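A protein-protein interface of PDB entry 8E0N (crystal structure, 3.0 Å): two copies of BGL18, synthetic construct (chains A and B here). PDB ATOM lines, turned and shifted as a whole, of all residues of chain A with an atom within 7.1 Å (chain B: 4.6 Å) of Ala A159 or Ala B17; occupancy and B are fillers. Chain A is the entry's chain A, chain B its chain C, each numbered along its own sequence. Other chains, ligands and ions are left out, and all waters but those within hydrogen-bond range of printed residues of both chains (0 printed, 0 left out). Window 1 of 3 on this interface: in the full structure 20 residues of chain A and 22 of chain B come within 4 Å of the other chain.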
ATOM      1  N   LEU A 125     -25.058 -11.363  -9.475  1.00  0.00           N
ATOM      2  CA  LEU A 125     -24.364 -10.765 -10.610  1.00  0.00           C
ATOM      3  C   LEU A 125     -22.865 -10.661 -10.366  1.00  0.00           C
ATOM      4  O   LEU A 125     -22.082 -10.700 -11.322  1.00  0.00           O
ATOM      5  CB  LEU A 125     -24.955  -9.389 -10.921  1.00  0.00           C
ATOM      6  CG  LEU A 125     -26.300  -9.373 -11.650  1.00  0.00           C
ATOM      7  CD1 LEU A 125     -26.908  -7.979 -11.625  1.00  0.00           C
ATOM      8  CD2 LEU A 125     -26.139  -9.871 -13.073  1.00  0.00           C
ATOM      9  N   ASN A 129     -19.324 -12.174 -12.724  1.00  0.00           N
ATOM     10  CA  ASN A 129     -17.966 -11.684 -12.945  1.00  0.00           C
ATOM     11  C   ASN A 129     -16.940 -12.735 -12.550  1.00  0.00           C
ATOM     12  O   ASN A 129     -15.991 -13.009 -13.292  1.00  0.00           O
ATOM     13  CB  ASN A 129     -17.732 -10.395 -12.156  1.00  0.00           C
ATOM     14  CG  ASN A 129     -18.011  -9.150 -12.971  1.00  0.00           C
ATOM     15  OD1 ASN A 129     -17.593  -9.043 -14.122  1.00  0.00           O
ATOM     16  ND2 ASN A 129     -18.718  -8.196 -12.372  1.00  0.00           N
ATOM     17  N   ARG A 133     -14.764 -14.300 -15.459  1.00  0.00           N
ATOM     18  CA  ARG A 133     -13.333 -14.021 -15.409  1.00  0.00           C
ATOM     19  C   ARG A 133     -12.525 -15.310 -15.479  1.00  0.00           C
ATOM     20  O   ARG A 133     -11.446 -15.341 -16.081  1.00  0.00           O
ATOM     21  CB  ARG A 133     -13.004 -13.238 -14.137  1.00  0.00           C
ATOM     22  CG  ARG A 133     -11.549 -12.830 -13.986  1.00  0.00           C
ATOM     23  CD  ARG A 133     -11.268 -12.413 -12.552  1.00  0.00           C
ATOM     24  NE  ARG A 133     -12.023 -11.222 -12.182  1.00  0.00           N
ATOM     25  CZ  ARG A 133     -11.491 -10.036 -11.920  1.00  0.00           C
ATOM     26  NH1 ARG A 133     -10.183  -9.838 -11.968  1.00  0.00           N
ATOM     27  NH2 ARG A 133     -12.291  -9.021 -11.603  1.00  0.00           N
ATOM     28  N   ARG A 153     -19.590 -11.551 -23.056  1.00  0.00           N
ATOM     29  CA  ARG A 153     -20.985 -11.170 -22.871  1.00  0.00           C
ATOM     30  C   ARG A 153     -21.397 -11.328 -21.414  1.00  0.00           C
ATOM     31  O   ARG A 153     -22.167 -10.516 -20.886  1.00  0.00           O
ATOM     32  CB  ARG A 153     -21.911 -12.012 -23.751  1.00  0.00           C
ATOM     33  CG  ARG A 153     -21.403 -12.385 -25.130  1.00  0.00           C
ATOM     34  CD  ARG A 153     -22.297 -13.483 -25.701  1.00  0.00           C
ATOM     35  NE  ARG A 153     -22.010 -13.805 -27.093  1.00  0.00           N
ATOM     36  CZ  ARG A 153     -21.665 -15.011 -27.524  1.00  0.00           C
ATOM     37  NH1 ARG A 153     -21.551 -16.034 -26.693  1.00  0.00           N
ATOM     38  NH2 ARG A 153     -21.437 -15.196 -28.821  1.00  0.00           N
ATOM     39  N   LEU A 154     -20.894 -12.376 -20.755  1.00  0.00           N
ATOM     40  CA  LEU A 154     -21.289 -12.656 -19.378  1.00  0.00           C
ATOM     41  C   LEU A 154     -20.866 -11.530 -18.445  1.00  0.00           C
ATOM     42  O   LEU A 154     -21.600 -11.175 -17.513  1.00  0.00           O
ATOM     43  CB  LEU A 154     -20.686 -13.987 -18.928  1.00  0.00           C
ATOM     44  CG  LEU A 154     -21.430 -15.255 -19.354  1.00  0.00           C
ATOM     45  CD1 LEU A 154     -20.949 -16.458 -18.555  1.00  0.00           C
ATOM     46  CD2 LEU A 154     -22.936 -15.081 -19.229  1.00  0.00           C
ATOM     47  N   THR A 155     -19.686 -10.953 -18.678  1.00  0.00           N
ATOM     48  CA  THR A 155     -19.245  -9.826 -17.865  1.00  0.00           C
ATOM     49  C   THR A 155     -20.085  -8.584 -18.143  1.00  0.00           C
ATOM     50  O   THR A 155     -20.447  -7.851 -17.214  1.00  0.00           O
ATOM     51  CB  THR A 155     -17.763  -9.550 -18.118  1.00  0.00           C
ATOM     52  OG1 THR A 155     -16.996 -10.718 -17.797  1.00  0.00           O
ATOM     53  CG2 THR A 155     -17.279  -8.396 -17.260  1.00  0.00           C
ATOM     54  N   HIS A 156     -20.413  -8.338 -19.415  1.00  0.00           N
ATOM     55  CA  HIS A 156     -21.258  -7.199 -19.762  1.00  0.00           C
ATOM     56  C   HIS A 156     -22.647  -7.317 -19.147  1.00  0.00           C
ATOM     57  O   HIS A 156     -23.241  -6.306 -18.759  1.00  0.00           O
ATOM     58  CB  HIS A 156     -21.356  -7.068 -21.282  1.00  0.00           C
ATOM     59  CG  HIS A 156     -20.488  -5.991 -21.857  1.00  0.00           C
ATOM     60  ND1 HIS A 156     -20.791  -4.652 -21.734  1.00  0.00           N
ATOM     61  CD2 HIS A 156     -19.324  -6.051 -22.546  1.00  0.00           C
ATOM     62  CE1 HIS A 156     -19.858  -3.935 -22.332  1.00  0.00           C
ATOM     63  NE2 HIS A 156     -18.954  -4.759 -22.832  1.00  0.00           N
ATOM     64  N   ARG A 157     -23.179  -8.538 -19.051  1.00  0.00           N
ATOM     65  CA  ARG A 157     -24.474  -8.750 -18.414  1.00  0.00           C
ATOM     66  C   ARG A 157     -24.424  -8.428 -16.927  1.00  0.00           C
ATOM     67  O   ARG A 157     -25.415  -7.952 -16.363  1.00  0.00           O
ATOM     68  CB  ARG A 157     -24.922 -10.191 -18.648  1.00  0.00           C
ATOM     69  CG  ARG A 157     -26.307 -10.539 -18.136  1.00  0.00           C
ATOM     70  CD  ARG A 157     -26.667 -11.947 -18.578  1.00  0.00           C
ATOM     71  NE  ARG A 157     -27.011 -11.979 -19.995  1.00  0.00           N
ATOM     72  CZ  ARG A 157     -26.904 -13.045 -20.778  1.00  0.00           C
ATOM     73  NH1 ARG A 157     -26.441 -14.197 -20.321  1.00  0.00           N
ATOM     74  NH2 ARG A 157     -27.265 -12.952 -22.056  1.00  0.00           N
ATOM     75  N   SER A 158     -23.283  -8.680 -16.283  1.00  0.00           N
ATOM     76  CA  SER A 158     -23.113  -8.275 -14.893  1.00  0.00           C
ATOM     77  C   SER A 158     -23.150  -6.761 -14.760  1.00  0.00           C
ATOM     78  O   SER A 158     -23.701  -6.226 -13.790  1.00  0.00           O
ATOM     79  CB  SER A 158     -21.798  -8.827 -14.347  1.00  0.00           C
ATOM     80  OG  SER A 158     -21.537  -8.323 -13.054  1.00  0.00           O
ATOM     81  N   ALA A 159     -22.568  -6.053 -15.729  1.00  0.00           N
ATOM     82  CA  ALA A 159     -22.550  -4.597 -15.686  1.00  0.00           C
ATOM     83  C   ALA A 159     -23.891  -4.014 -16.109  1.00  0.00           C
ATOM     84  O   ALA A 159     -24.406  -3.090 -15.467  1.00  0.00           O
ATOM     85  CB  ALA A 159     -21.430  -4.064 -16.580  1.00  0.00           C
ATOM     86  N   LYS A 160     -24.471  -4.548 -17.186  1.00  0.00           N
ATOM     87  CA  LYS A 160     -25.720  -4.001 -17.705  1.00  0.00           C
ATOM     88  C   LYS A 160     -26.872  -4.223 -16.733  1.00  0.00           C
ATOM     89  O   LYS A 160     -27.676  -3.313 -16.499  1.00  0.00           O
ATOM     90  CB  LYS A 160     -26.038  -4.624 -19.065  1.00  0.00           C
ATOM     91  N   TRP A 161     -26.971  -5.424 -16.157  1.00  0.00           N
ATOM     92  CA  TRP A 161     -28.055  -5.692 -15.219  1.00  0.00           C
ATOM     93  C   TRP A 161     -27.858  -4.955 -13.902  1.00  0.00           C
ATOM     94  O   TRP A 161     -28.839  -4.633 -13.225  1.00  0.00           O
ATOM     95  CB  TRP A 161     -28.194  -7.195 -14.979  1.00  0.00           C
ATOM     96  CG  TRP A 161     -28.834  -7.921 -16.125  1.00  0.00           C
ATOM     97  CD1 TRP A 161     -29.134  -7.407 -17.353  1.00  0.00           C
ATOM     98  CD2 TRP A 161     -29.272  -9.285 -16.144  1.00  0.00           C
ATOM     99  NE1 TRP A 161     -29.722  -8.368 -18.138  1.00  0.00           N
ATOM    100  CE2 TRP A 161     -29.820  -9.529 -17.419  1.00  0.00           C
ATOM    101  CE3 TRP A 161     -29.252 -10.324 -15.209  1.00  0.00           C
ATOM    102  CZ2 TRP A 161     -30.341 -10.770 -17.782  1.00  0.00           C
ATOM    103  CZ3 TRP A 161     -29.771 -11.555 -15.571  1.00  0.00           C
ATOM    104  CH2 TRP A 161     -30.308 -11.767 -16.848  1.00  0.00           C
ATOM    105  N   SER A 162     -26.608  -4.671 -13.525  1.00  0.00           N
ATOM    106  CA  SER A 162     -26.371  -3.897 -12.311  1.00  0.00           C
ATOM    107  C   SER A 162     -26.755  -2.436 -12.505  1.00  0.00           C
ATOM    108  O   SER A 162     -27.295  -1.803 -11.590  1.00  0.00           O
ATOM    109  CB  SER A 162     -24.907  -4.013 -11.891  1.00  0.00           C
ATOM    110  OG  SER A 162     -24.593  -5.341 -11.509  1.00  0.00           O
ATOM    111  N   ARG A 163     -26.480  -1.886 -13.691  1.00  0.00           N
ATOM    112  CA  ARG A 163     -26.834  -0.497 -13.971  1.00  0.00           C
ATOM    113  C   ARG A 163     -28.339  -0.282 -13.890  1.00  0.00           C
ATOM    114  O   ARG A 163     -28.801   0.752 -13.393  1.00  0.00           O
ATOM    115  CB  ARG A 163     -26.321  -0.095 -15.351  1.00  0.00           C
ATOM    116  CG  ARG A 163     -26.574   1.357 -15.710  1.00  0.00           C
ATOM    117  CD  ARG A 163     -25.722   1.764 -16.893  1.00  0.00           C
ATOM    118  NE  ARG A 163     -25.579   0.667 -17.842  1.00  0.00           N
ATOM    119  CZ  ARG A 163     -24.520   0.481 -18.618  1.00  0.00           C
ATOM    120  NH1 ARG A 163     -23.488   1.305 -18.586  1.00  0.00           N
ATOM    121  NH2 ARG A 163     -24.498  -0.561 -19.446  1.00  0.00           N
ATOM    122  N   GLU A 164     -29.118  -1.244 -14.385  1.00  0.00           N
ATOM    123  CA  GLU A 164     -30.571  -1.126 -14.322  1.00  0.00           C
ATOM    124  C   GLU A 164     -31.049  -1.114 -12.876  1.00  0.00           C
ATOM    125  O   GLU A 164     -31.900  -0.299 -12.498  1.00  0.00           O
ATOM    126  CB  GLU A 164     -31.214  -2.272 -15.101  1.00  0.00           C
ATOM    127  CG  GLU A 164     -30.889  -2.274 -16.589  1.00  0.00           C
ATOM    128  CD  GLU A 164     -31.333  -3.551 -17.283  1.00  0.00           C
ATOM    129  OE1 GLU A 164     -32.125  -4.310 -16.688  1.00  0.00           O
ATOM    130  OE2 GLU A 164     -30.888  -3.796 -18.424  1.00  0.00           O
ATOM    131  N   ILE A 165     -30.504  -2.006 -12.046  1.00  0.00           N
ATOM    132  CA  ILE A 165     -30.821  -1.985 -10.621  1.00  0.00           C
ATOM    133  C   ILE A 165     -30.291  -0.715  -9.966  1.00  0.00           C
ATOM    134  O   ILE A 165     -30.848  -0.246  -8.965  1.00  0.00           O
ATOM    135  CB  ILE A 165     -30.272  -3.246  -9.929  1.00  0.00           C
ATOM    136  CG1 ILE A 165     -30.637  -4.496 -10.733  1.00  0.00           C
ATOM    137  CG2 ILE A 165     -30.797  -3.354  -8.508  1.00  0.00           C
ATOM    138  CD1 ILE A 165     -30.218  -5.784 -10.072  1.00  0.00           C
ATOM    139  N   ASN B  13     -20.502  -3.531  -8.574  1.00  0.00           N
ATOM    140  CA  ASN B  13     -20.508  -4.570  -9.596  1.00  0.00           C
ATOM    141  C   ASN B  13     -19.992  -4.049 -10.929  1.00  0.00           C
ATOM    142  O   ASN B  13     -19.459  -4.824 -11.730  1.00  0.00           O
ATOM    143  CB  ASN B  13     -21.921  -5.125  -9.758  1.00  0.00           C
ATOM    144  CG  ASN B  13     -22.279  -6.132  -8.682  1.00  0.00           C
ATOM    145  OD1 ASN B  13     -21.523  -6.339  -7.733  1.00  0.00           O
ATOM    146  ND2 ASN B  13     -23.445  -6.754  -8.821  1.00  0.00           N
ATOM    147  N   MET B  14     -20.127  -2.746 -11.182  1.00  0.00           N
ATOM    148  CA  MET B  14     -19.800  -2.218 -12.500  1.00  0.00           C
ATOM    149  C   MET B  14     -18.305  -1.975 -12.672  1.00  0.00           C
ATOM    150  O   MET B  14     -17.793  -2.093 -13.791  1.00  0.00           O
ATOM    151  CB  MET B  14     -20.599  -0.938 -12.758  1.00  0.00           C
ATOM    152  CG  MET B  14     -22.107  -1.178 -12.833  1.00  0.00           C
ATOM    153  SD  MET B  14     -23.076   0.239 -13.390  1.00  0.00           S
ATOM    154  CE  MET B  14     -21.909   1.054 -14.476  1.00  0.00           C
ATOM    155  N   VAL B  15     -17.586  -1.645 -11.594  1.00  0.00           N
ATOM    156  CA  VAL B  15     -16.129  -1.587 -11.686  1.00  0.00           C
ATOM    157  C   VAL B  15     -15.546  -2.987 -11.814  1.00  0.00           C
ATOM    158  O   VAL B  15     -14.593  -3.208 -12.572  1.00  0.00           O
ATOM    159  CB  VAL B  15     -15.526  -0.839 -10.482  1.00  0.00           C
ATOM    160  CG1 VAL B  15     -15.743   0.645 -10.616  1.00  0.00           C
ATOM    161  CG2 VAL B  15     -16.132  -1.342  -9.181  1.00  0.00           C
ATOM    162  N   ARG B  16     -16.102  -3.951 -11.074  1.00  0.00           N
ATOM    163  CA  ARG B  16     -15.626  -5.326 -11.166  1.00  0.00           C
ATOM    164  C   ARG B  16     -15.775  -5.858 -12.583  1.00  0.00           C
ATOM    165  O   ARG B  16     -14.941  -6.641 -13.054  1.00  0.00           O
ATOM    166  CB  ARG B  16     -16.386  -6.206 -10.174  1.00  0.00           C
ATOM    167  CG  ARG B  16     -15.614  -6.531  -8.907  1.00  0.00           C
ATOM    168  CD  ARG B  16     -16.412  -7.448  -7.997  1.00  0.00           C
ATOM    169  NE  ARG B  16     -17.308  -6.700  -7.124  1.00  0.00           N
ATOM    170  CZ  ARG B  16     -16.957  -6.185  -5.953  1.00  0.00           C
ATOM    171  NH1 ARG B  16     -15.727  -6.313  -5.483  1.00  0.00           N
ATOM    172  NH2 ARG B  16     -17.862  -5.524  -5.235  1.00  0.00           N
ATOM    173  N   ALA B  17     -16.831  -5.438 -13.281  1.00  0.00           N
ATOM    174  CA  ALA B  17     -16.981  -5.798 -14.686  1.00  0.00           C
ATOM    175  C   ALA B  17     -16.009  -5.009 -15.553  1.00  0.00           C
ATOM    176  O   ALA B  17     -15.360  -5.570 -16.444  1.00  0.00           O
ATOM    177  CB  ALA B  17     -18.422  -5.565 -15.136  1.00  0.00           C
ATOM    178  N   ALA B  18     -15.893  -3.701 -15.301  1.00  0.00           N
ATOM    179  CA  ALA B  18     -14.966  -2.876 -16.069  1.00  0.00           C
ATOM    180  C   ALA B  18     -13.530  -3.349 -15.893  1.00  0.00           C
ATOM    181  O   ALA B  18     -12.740  -3.332 -16.845  1.00  0.00           O
ATOM    182  CB  ALA B  18     -15.104  -1.410 -15.659  1.00  0.00           C
ATOM    183  N   HIS B  19     -13.175  -3.778 -14.680  1.00  0.00           N
ATOM    184  CA  HIS B  19     -11.862  -4.374 -14.462  1.00  0.00           C
ATOM    185  C   HIS B  19     -11.743  -5.713 -15.178  1.00  0.00           C
ATOM    186  O   HIS B  19     -10.689  -6.034 -15.739  1.00  0.00           O
ATOM    187  CB  HIS B  19     -11.606  -4.543 -12.965  1.00  0.00           C
ATOM    188  CG  HIS B  19     -10.324  -5.247 -12.647  1.00  0.00           C
ATOM    189  ND1 HIS B  19     -10.280  -6.426 -11.934  1.00  0.00           N
ATOM    190  CD2 HIS B  19      -9.038  -4.936 -12.936  1.00  0.00           C
ATOM    191  CE1 HIS B  19      -9.024  -6.813 -11.803  1.00  0.00           C
ATOM    192  NE2 HIS B  19      -8.251  -5.926 -12.403  1.00  0.00           N
ATOM    193  N   THR B  20     -12.814  -6.510 -15.165  1.00  0.00           N
ATOM    194  CA  THR B  20     -12.797  -7.784 -15.875  1.00  0.00           C
ATOM    195  C   THR B  20     -12.745  -7.570 -17.382  1.00  0.00           C
ATOM    196  O   THR B  20     -12.031  -8.287 -18.093  1.00  0.00           O
ATOM    197  CB  THR B  20     -14.023  -8.615 -15.492  1.00  0.00           C
ATOM    198  OG1 THR B  20     -14.090  -8.741 -14.066  1.00  0.00           O
ATOM    199  CG2 THR B  20     -13.948 -10.003 -16.113  1.00  0.00           C
ATOM    200  N   LEU B  21     -13.493  -6.585 -17.886  1.00  0.00           N
ATOM    201  CA  LEU B  21     -13.474  -6.286 -19.314  1.00  0.00           C
ATOM    202  C   LEU B  21     -12.085  -5.853 -19.768  1.00  0.00           C
ATOM    203  O   LEU B  21     -11.574  -6.337 -20.785  1.00  0.00           O
ATOM    204  CB  LEU B  21     -14.513  -5.208 -19.633  1.00  0.00           C
ATOM    205  CG  LEU B  21     -15.990  -5.605 -19.642  1.00  0.00           C
ATOM    206  CD1 LEU B  21     -16.811  -4.535 -20.336  1.00  0.00           C
ATOM    207  CD2 LEU B  21     -16.159  -6.937 -20.353  1.00  0.00           C
ATOM    208  N   LEU B  40     -16.847   1.996 -19.997  1.00  0.00           N
ATOM    209  CA  LEU B  40     -17.598   1.569 -18.822  1.00  0.00           C
ATOM    210  C   LEU B  40     -17.001   2.151 -17.546  1.00  0.00           C
ATOM    211  O   LEU B  40     -17.737   2.618 -16.668  1.00  0.00           O
ATOM    212  CB  LEU B  40     -17.638   0.042 -18.757  1.00  0.00           C
ATOM    213  CG  LEU B  40     -18.291  -0.588 -17.525  1.00  0.00           C
ATOM    214  CD1 LEU B  40     -19.667   0.009 -17.274  1.00  0.00           C
ATOM    215  CD2 LEU B  40     -18.378  -2.101 -17.681  1.00  0.00           C
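Asn B13 touches Leu A125 (ND2 to CB, 3.7 Å).
Asn A129 touches Asn B13.
Asn A129 touches Arg B16 (OD1 to O, 3.7 Å).
OG1 of Thr B20 touches OD1 of Asn A129 (3.5 Å).
Arg B16 touches Arg A133 (O to NH2, 3.8 Å).
CG2 of Thr A155 touches O of Ala B17 (3.5 Å).
Thr A155 touches Leu B21 (CG2 to CD2, 3.6 Å).
Ala A159 touches Met B14 (O to CG, 3.98 Å).
Ala A159 touches Leu B40.
Met B14 touches Arg A163 (SD to CB, 3.8 Å).
The guanidinium group of Arg A133 sits at hydrogen-bond distance from the side-chain hydroxyl of Thr B20 (3.1 Å).
The side-chain amide nitrogen (ND2) of Asn A129 lies close to the backbone NH (N) of Ala B17 (3.5 Å).
The side-chain amide nitrogen (ND2) of Asn B13 sits close to the side-chain hydroxyl (OG) of Ser A162.
A ring nitrogen (ND1) of His B19 sits at hydrogen-bond distance from the guanidinium group (NH2) of Arg A133, 3.3 Å away.
Of the 16 printed residues of chain A, 8 touch a printed residue of chain B.
Hydrophobic or aromatic side chains of chain A that line the printed part of chain B: Leu A125, His A156 and Ala A159.
Hydrophobic or aromatic side chains of chain B that line the printed part of chain A: Met B14, Ala B17, His B19, Leu B21 and Leu B40.
Of the printed residues of chain B, Thr A155 touches Ala B17 (3.5 Å), Thr B20 (3.6 Å) and Leu B21 (3.6 Å).
Of the printed residues of chain B, Ala A159 touches Met B14, Ala B17 and Leu B40.
Glu A164 touches none of the printed residues of chain B.
Val B15 touches none of the printed residues of chain A.
Ala B17 touches three residues of chain A.
Of the printed residues of chain A, His B19 touches Arg A133 (3.2 Å).
The nearest printed residue of chain B that does not touch Ala A159 is Asn B13 (5.0 Å).
The nearest residue of chain A that does not touch Ala B17 is Ser A158 (4.7 Å).
No position is printed for both chains.
Of the 17 pairs that touch across the chains among the printed residues, none has its exchanged pair printed and touching as well.
O of Arg B16 is in hydrogen-bond range of OG1 of Thr B20.
The side-chain hydroxyl (OG) of Ser A158 lies within hydrogen-bond range of the side-chain amide nitrogen (ND2) of Asn A129 (2.9 Å).
The backbone carbonyl oxygen (O) of Ser A158 is in hydrogen-bond range of the side-chain hydroxyl (OG) of Ser A162 (2.6 Å).
The backbone carbonyl oxygen (O) of Leu A125 sits at hydrogen-bond distance from the side-chain hydroxyl (OG) of Ser A158.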
